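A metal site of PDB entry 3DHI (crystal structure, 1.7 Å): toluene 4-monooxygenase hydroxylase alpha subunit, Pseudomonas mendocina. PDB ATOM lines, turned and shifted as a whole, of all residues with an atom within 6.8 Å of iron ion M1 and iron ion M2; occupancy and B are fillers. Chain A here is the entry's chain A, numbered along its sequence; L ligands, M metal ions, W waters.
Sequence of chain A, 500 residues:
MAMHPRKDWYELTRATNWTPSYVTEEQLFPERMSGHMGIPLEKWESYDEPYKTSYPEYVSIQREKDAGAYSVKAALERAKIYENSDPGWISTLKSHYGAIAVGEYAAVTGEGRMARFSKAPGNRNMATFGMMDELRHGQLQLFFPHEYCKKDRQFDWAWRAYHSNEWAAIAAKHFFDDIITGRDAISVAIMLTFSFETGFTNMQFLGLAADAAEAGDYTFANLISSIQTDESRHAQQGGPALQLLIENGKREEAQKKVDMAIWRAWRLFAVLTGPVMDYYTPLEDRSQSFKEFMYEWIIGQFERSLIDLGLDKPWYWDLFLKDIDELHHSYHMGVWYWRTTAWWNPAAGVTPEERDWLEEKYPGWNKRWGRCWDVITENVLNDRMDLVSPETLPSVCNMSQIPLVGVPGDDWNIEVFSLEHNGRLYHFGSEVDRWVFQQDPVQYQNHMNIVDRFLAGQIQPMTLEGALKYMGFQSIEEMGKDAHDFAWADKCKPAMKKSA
Of the 21 residues printed, 4 come within 4 Å of iron ion M1. Along chain A the residues within 4 Å of iron ion M1 span positions 104 to 231.
Iron ion M2 is bound by the side-chain carboxylate (OE2) of Glu 197 (2.1 Å), the side-chain carboxylate (OE2) of Glu 134 (2.1 Å), the side-chain carboxylate (OE2) of Glu 231 (2.1 Å), a ring nitrogen (NE2) of His 234 (2.1 Å), an oxygen (O2) of the ligand (2.2 Å) and the side-chain carboxylate (OE1) of Glu 231 (2.3 Å). Iron ion M2 has six donor atoms within binding distance. Slightly farther from iron ion M2 lies an oxygen (O1) of the ligand (2.8 Å).
Of the 21 residues printed, 4 come within 4 Å of iron ion M2. The nearest printed residue that does not touch iron ion M2 is Glu 111 (4.9 Å).
OE1 of Glu 134 is bound to iron ion M1 (2.1 Å). Iron ion M1 is bound by OE2 of Glu 104 (2.1 Å). Iron ion M1 is bound by water W1 (2.2 Å). An oxygen (O1) of the ligand is bound to iron ion M1. The side-chain carboxylate (OE1) of Glu 231 is bound to iron ion M1, at 2.2 Å. A ring nitrogen (ND1) of His 137 is bound to iron ion M1 (2.3 Å).
The backbone carbonyl oxygen (O) of Leu 192 lies within hydrogen-bond range of the backbone NH (N) of Glu 197 (2.9 Å). The backbone carbonyl oxygen (O) of Glu 197 sits at hydrogen-bond distance from the side-chain hydroxyl (OG1) of Thr 201, 3.2 Å away. OE1 of Glu 104 sits close to OE1 of Gln 141 (2.9 Å). A ring nitrogen (ND1) of His 234 is in hydrogen-bond range of the backbone carbonyl oxygen of Asp 230. A ring nitrogen (NE2) of His 137 lies within hydrogen-bond range of the backbone carbonyl oxygen of Ile 227, at 3.4 Å. A ring nitrogen (NE2) of His 137 lies close to the backbone carbonyl oxygen (O) of Asp 133, 3.4 Å away. OE1 of Gln 141 sits close to O of His 137 (3.1 Å). NE2 of His 137 is in hydrogen-bond range of OD2 of Asp 230 (2.7 Å).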
ATOM      1  N   GLU A 104      11.006   4.789   1.200  1.00  0.00           N
ATOM      2  CA  GLU A 104      12.021   4.867   0.137  1.00  0.00           C
ATOM      3  C   GLU A 104      13.252   5.555   0.681  1.00  0.00           C
ATOM      4  O   GLU A 104      14.351   5.114   0.451  1.00  0.00           O
ATOM      5  CB  GLU A 104      11.527   5.691  -1.071  1.00  0.00           C
ATOM      6  CG  GLU A 104      10.377   5.070  -1.810  1.00  0.00           C
ATOM      7  CD  GLU A 104      10.806   4.132  -2.920  1.00  0.00           C
ATOM      8  OE1 GLU A 104       9.988   3.868  -3.806  1.00  0.00           O
ATOM      9  OE2 GLU A 104      11.962   3.658  -2.901  1.00  0.00           O
ATOM     10  N   ALA A 107      15.221   3.263   2.693  1.00  0.00           N
ATOM     11  CA  ALA A 107      15.977   2.324   1.859  1.00  0.00           C
ATOM     12  C   ALA A 107      17.361   2.836   1.490  1.00  0.00           C
ATOM     13  O   ALA A 107      18.255   2.037   1.232  1.00  0.00           O
ATOM     14  CB  ALA A 107      15.188   1.945   0.590  1.00  0.00           C
ATOM     15  N   GLU A 111      20.889   0.530   1.496  1.00  0.00           N
ATOM     16  CA  GLU A 111      21.929   0.592   0.468  1.00  0.00           C
ATOM     17  C   GLU A 111      23.246   1.065   1.086  1.00  0.00           C
ATOM     18  O   GLU A 111      24.314   0.506   0.764  1.00  0.00           O
ATOM     19  CB  GLU A 111      21.504   1.489  -0.686  1.00  0.00           C
ATOM     20  CG  GLU A 111      20.268   0.939  -1.446  1.00  0.00           C
ATOM     21  CD  GLU A 111      20.553  -0.304  -2.296  1.00  0.00           C
ATOM     22  OE1 GLU A 111      21.699  -0.509  -2.738  1.00  0.00           O
ATOM     23  OE2 GLU A 111      19.612  -1.112  -2.542  1.00  0.00           O
ATOM     24  N   GLY A 130      22.666   2.500  -5.647  1.00  0.00           N
ATOM     25  CA  GLY A 130      21.396   2.193  -4.939  1.00  0.00           C
ATOM     26  C   GLY A 130      21.014   3.286  -3.954  1.00  0.00           C
ATOM     27  O   GLY A 130      19.868   3.676  -3.867  1.00  0.00           O
ATOM     28  N   ASP A 133      19.677   6.034  -6.020  1.00  0.00           N
ATOM     29  CA  ASP A 133      18.346   5.650  -6.539  1.00  0.00           C
ATOM     30  C   ASP A 133      17.252   5.860  -5.485  1.00  0.00           C
ATOM     31  O   ASP A 133      16.166   6.398  -5.780  1.00  0.00           O
ATOM     32  CB  ASP A 133      18.309   4.162  -6.930  1.00  0.00           C
ATOM     33  CG  ASP A 133      19.130   3.844  -8.198  1.00  0.00           C
ATOM     34  OD1 ASP A 133      19.452   4.744  -8.996  1.00  0.00           O
ATOM     35  OD2 ASP A 133      19.449   2.661  -8.378  1.00  0.00           O
ATOM     36  N   GLU A 134      17.504   5.393  -4.258  1.00  0.00           N
ATOM     37  CA  GLU A 134      16.466   5.523  -3.232  1.00  0.00           C
ATOM     38  C   GLU A 134      16.289   6.967  -2.800  1.00  0.00           C
ATOM     39  O   GLU A 134      15.175   7.353  -2.451  1.00  0.00           O
ATOM     40  CB  GLU A 134      16.744   4.665  -2.019  1.00  0.00           C
ATOM     41  CG  GLU A 134      17.043   3.199  -2.317  1.00  0.00           C
ATOM     42  CD  GLU A 134      15.866   2.436  -2.903  1.00  0.00           C
ATOM     43  OE1 GLU A 134      14.866   3.013  -3.384  1.00  0.00           O
ATOM     44  OE2 GLU A 134      15.959   1.199  -2.885  1.00  0.00           O
ATOM     45  N   HIS A 137      13.915   8.187  -5.223  1.00  0.00           N
ATOM     46  CA  HIS A 137      12.544   7.676  -5.041  1.00  0.00           C
ATOM     47  C   HIS A 137      11.848   8.370  -3.888  1.00  0.00           C
ATOM     48  O   HIS A 137      10.664   8.663  -4.002  1.00  0.00           O
ATOM     49  CB  HIS A 137      12.554   6.171  -4.825  1.00  0.00           C
ATOM     50  CG  HIS A 137      13.167   5.429  -5.976  1.00  0.00           C
ATOM     51  ND1 HIS A 137      13.495   4.096  -5.907  1.00  0.00           N
ATOM     52  CD2 HIS A 137      13.529   5.839  -7.218  1.00  0.00           C
ATOM     53  CE1 HIS A 137      14.036   3.718  -7.069  1.00  0.00           C
ATOM     54  NE2 HIS A 137      14.065   4.755  -7.880  1.00  0.00           N
ATOM     55  N   GLY A 138      12.590   8.642  -2.808  1.00  0.00           N
ATOM     56  CA  GLY A 138      12.018   9.379  -1.665  1.00  0.00           C
ATOM     57  C   GLY A 138      11.641  10.797  -2.071  1.00  0.00           C
ATOM     58  O   GLY A 138      10.555  11.296  -1.722  1.00  0.00           O
ATOM     59  N   GLN A 141       8.644  10.939  -4.472  1.00  0.00           N
ATOM     60  CA  GLN A 141       7.389  10.548  -3.844  1.00  0.00           C
ATOM     61  C   GLN A 141       6.945  11.468  -2.677  1.00  0.00           C
ATOM     62  O   GLN A 141       5.861  11.277  -2.143  1.00  0.00           O
ATOM     63  CB  GLN A 141       7.401   9.059  -3.496  1.00  0.00           C
ATOM     64  CG  GLN A 141       7.256   8.256  -4.790  1.00  0.00           C
ATOM     65  CD  GLN A 141       7.520   6.797  -4.634  1.00  0.00           C
ATOM     66  OE1 GLN A 141       8.631   6.363  -4.253  1.00  0.00           O
ATOM     67  NE2 GLN A 141       6.520   6.009  -4.991  1.00  0.00           N
ATOM     68  N   LEU A 192      16.247  -7.478   1.103  1.00  0.00           N
ATOM     69  CA  LEU A 192      15.672  -6.289   0.488  1.00  0.00           C
ATOM     70  C   LEU A 192      15.751  -6.459  -1.021  1.00  0.00           C
ATOM     71  O   LEU A 192      14.734  -6.451  -1.697  1.00  0.00           O
ATOM     72  CB  LEU A 192      16.392  -4.998   0.916  1.00  0.00           C
ATOM     73  CG  LEU A 192      16.129  -3.727   0.096  1.00  0.00           C
ATOM     74  CD1 LEU A 192      14.653  -3.384   0.077  1.00  0.00           C
ATOM     75  CD2 LEU A 192      16.928  -2.590   0.746  1.00  0.00           C
ATOM     76  N   THR A 193      16.982  -6.595  -1.543  1.00  0.00           N
ATOM     77  CA  THR A 193      17.175  -6.399  -2.966  1.00  0.00           C
ATOM     78  C   THR A 193      16.687  -7.627  -3.679  1.00  0.00           C
ATOM     79  O   THR A 193      15.850  -7.540  -4.581  1.00  0.00           O
ATOM     80  CB  THR A 193      18.633  -6.012  -3.382  1.00  0.00           C
ATOM     81  OG1 THR A 193      19.511  -7.101  -3.122  1.00  0.00           O
ATOM     82  CG2 THR A 193      19.128  -4.764  -2.644  1.00  0.00           C
ATOM     83  N   PHE A 196      12.462  -8.555  -1.570  1.00  0.00           N
ATOM     84  CA  PHE A 196      11.510  -7.441  -1.766  1.00  0.00           C
ATOM     85  C   PHE A 196      11.485  -6.706  -3.148  1.00  0.00           C
ATOM     86  O   PHE A 196      10.388  -6.474  -3.690  1.00  0.00           O
ATOM     87  CB  PHE A 196      11.640  -6.437  -0.613  1.00  0.00           C
ATOM     88  CG  PHE A 196      10.528  -5.440  -0.539  1.00  0.00           C
ATOM     89  CD1 PHE A 196       9.216  -5.839  -0.346  1.00  0.00           C
ATOM     90  CD2 PHE A 196      10.816  -4.081  -0.637  1.00  0.00           C
ATOM     91  CE1 PHE A 196       8.208  -4.902  -0.265  1.00  0.00           C
ATOM     92  CE2 PHE A 196       9.817  -3.140  -0.546  1.00  0.00           C
ATOM     93  CZ  PHE A 196       8.504  -3.535  -0.375  1.00  0.00           C
ATOM     94  N   GLU A 197      12.647  -6.341  -3.687  1.00  0.00           N
ATOM     95  CA  GLU A 197      12.756  -5.470  -4.876  1.00  0.00           C
ATOM     96  C   GLU A 197      12.599  -6.175  -6.228  1.00  0.00           C
ATOM     97  O   GLU A 197      12.373  -5.487  -7.258  1.00  0.00           O
ATOM     98  CB  GLU A 197      14.094  -4.707  -4.891  1.00  0.00           C
ATOM     99  CG  GLU A 197      14.361  -3.867  -3.668  1.00  0.00           C
ATOM    100  CD  GLU A 197      15.714  -3.186  -3.721  1.00  0.00           C
ATOM    101  OE1 GLU A 197      16.699  -3.813  -4.150  1.00  0.00           O
ATOM    102  OE2 GLU A 197      15.800  -2.003  -3.357  1.00  0.00           O
ATOM    103  N   THR A 201       7.748  -5.360  -5.100  1.00  0.00           N
ATOM    104  CA  THR A 201       7.608  -3.976  -5.576  1.00  0.00           C
ATOM    105  C   THR A 201       7.021  -3.908  -6.988  1.00  0.00           C
ATOM    106  O   THR A 201       6.345  -2.930  -7.338  1.00  0.00           O
ATOM    107  CB  THR A 201       8.905  -3.142  -5.497  1.00  0.00           C
ATOM    108  OG1 THR A 201       9.907  -3.766  -6.259  1.00  0.00           O
ATOM    109  CG2 THR A 201       9.340  -3.003  -4.063  1.00  0.00           C
ATOM    110  N   PHE A 205       4.273  -1.054  -8.059  1.00  0.00           N
ATOM    111  CA  PHE A 205       4.810  -0.075  -8.959  1.00  0.00           C
ATOM    112  C   PHE A 205       4.596  -0.365 -10.451  1.00  0.00           C
ATOM    113  O   PHE A 205       4.894   0.448 -11.277  1.00  0.00           O
ATOM    114  CB  PHE A 205       6.266   0.140  -8.714  1.00  0.00           C
ATOM    115  CG  PHE A 205       6.569   0.862  -7.446  1.00  0.00           C
ATOM    116  CD1 PHE A 205       6.382   0.288  -6.238  1.00  0.00           C
ATOM    117  CD2 PHE A 205       7.043   2.119  -7.480  1.00  0.00           C
ATOM    118  CE1 PHE A 205       6.667   0.971  -5.096  1.00  0.00           C
ATOM    119  CE2 PHE A 205       7.329   2.799  -6.347  1.00  0.00           C
ATOM    120  CZ  PHE A 205       7.136   2.201  -5.143  1.00  0.00           C
ATOM    121  N   ILE A 227      10.324   4.857 -11.581  1.00  0.00           N
ATOM    122  CA  ILE A 227      10.975   4.430 -10.358  1.00  0.00           C
ATOM    123  C   ILE A 227      11.404   2.970 -10.438  1.00  0.00           C
ATOM    124  O   ILE A 227      12.530   2.608 -10.077  1.00  0.00           O
ATOM    125  CB  ILE A 227      10.032   4.680  -9.167  1.00  0.00           C
ATOM    126  CG1 ILE A 227       9.978   6.191  -8.887  1.00  0.00           C
ATOM    127  CG2 ILE A 227      10.497   3.906  -7.943  1.00  0.00           C
ATOM    128  CD1 ILE A 227       9.061   6.609  -7.754  1.00  0.00           C
ATOM    129  N   GLN A 228      10.531   2.123 -10.983  1.00  0.00           N
ATOM    130  CA  GLN A 228      10.822   0.695 -11.033  1.00  0.00           C
ATOM    131  C   GLN A 228      12.021   0.336 -11.939  1.00  0.00           C
ATOM    132  O   GLN A 228      12.671  -0.689 -11.732  1.00  0.00           O
ATOM    133  CB  GLN A 228       9.579  -0.105 -11.401  1.00  0.00           C
ATOM    134  CG  GLN A 228       9.652  -1.566 -10.926  1.00  0.00           C
ATOM    135  CD  GLN A 228       9.677  -1.711  -9.409  1.00  0.00           C
ATOM    136  OE1 GLN A 228       9.632  -0.719  -8.650  1.00  0.00           O
ATOM    137  NE2 GLN A 228       9.739  -2.965  -8.940  1.00  0.00           N
ATOM    138  N   ASP A 230      14.788   1.870 -11.938  1.00  0.00           N
ATOM    139  CA  ASP A 230      15.970   1.895 -11.040  1.00  0.00           C
ATOM    140  C   ASP A 230      16.026   0.644 -10.188  1.00  0.00           C
ATOM    141  O   ASP A 230      17.081   0.044  -9.979  1.00  0.00           O
ATOM    142  CB  ASP A 230      15.913   3.091 -10.080  1.00  0.00           C
ATOM    143  CG  ASP A 230      15.897   4.426 -10.778  1.00  0.00           C
ATOM    144  OD1 ASP A 230      16.561   4.583 -11.829  1.00  0.00           O
ATOM    145  OD2 ASP A 230      15.232   5.363 -10.244  1.00  0.00           O
ATOM    146  N   GLU A 231      14.868   0.258  -9.653  1.00  0.00           N
ATOM    147  CA  GLU A 231      14.768  -0.927  -8.791  1.00  0.00           C
ATOM    148  C   GLU A 231      15.289  -2.112  -9.570  1.00  0.00           C
ATOM    149  O   GLU A 231      16.042  -2.930  -9.046  1.00  0.00           O
ATOM    150  CB  GLU A 231      13.314  -1.184  -8.402  1.00  0.00           C
ATOM    151  CG  GLU A 231      12.764  -0.122  -7.401  1.00  0.00           C
ATOM    152  CD  GLU A 231      13.553  -0.097  -6.106  1.00  0.00           C
ATOM    153  OE1 GLU A 231      13.931   1.016  -5.644  1.00  0.00           O
ATOM    154  OE2 GLU A 231      13.889  -1.174  -5.557  1.00  0.00           O
ATOM    155  N   HIS A 234      19.234  -1.903  -9.382  1.00  0.00           N
ATOM    156  CA  HIS A 234      19.906  -2.113  -8.084  1.00  0.00           C
ATOM    157  C   HIS A 234      19.483  -3.394  -7.357  1.00  0.00           C
ATOM    158  O   HIS A 234      20.224  -3.930  -6.507  1.00  0.00           O
ATOM    159  CB  HIS A 234      19.936  -0.855  -7.192  1.00  0.00           C
ATOM    160  CG  HIS A 234      18.608  -0.428  -6.619  1.00  0.00           C
ATOM    161  ND1 HIS A 234      18.104   0.841  -6.819  1.00  0.00           N
ATOM    162  CD2 HIS A 234      17.752  -1.045  -5.774  1.00  0.00           C
ATOM    163  CE1 HIS A 234      16.961   0.969  -6.169  1.00  0.00           C
ATOM    164  NE2 HIS A 234      16.729  -0.155  -5.513  1.00  0.00           N
ATOM    165  N   ALA A 235      18.299  -3.916  -7.688  1.00  0.00           N
ATOM    166  CA  ALA A 235      17.860  -5.195  -7.128  1.00  0.00           C
ATOM    167  C   ALA A 235      18.788  -6.355  -7.522  1.00  0.00           C
ATOM    168  O   ALA A 235      18.824  -7.388  -6.856  1.00  0.00           O
ATOM    169  CB  ALA A 235      16.424  -5.495  -7.536  1.00  0.00           C
HETATM  170  C1  LIG L   1      12.917  -0.093  -2.139  1.00  0.00           C
HETATM  171  O1  LIG L   1      12.819   0.874  -2.912  1.00  0.00           O
HETATM  172  O2  LIG L   1      13.821  -0.899  -2.425  1.00  0.00           O
HETATM  173  C2  LIG L   1      12.038  -0.264  -0.942  1.00  0.00           C
HETATM  174 FE    FE M   1      13.076   2.553  -4.316  1.00  0.00          FE
HETATM  175 FE    FE M   2      15.102  -0.224  -4.120  1.00  0.00          FE
HETATM  176  O   HOH W   1      11.107   2.031  -5.149  1.00  0.00           O
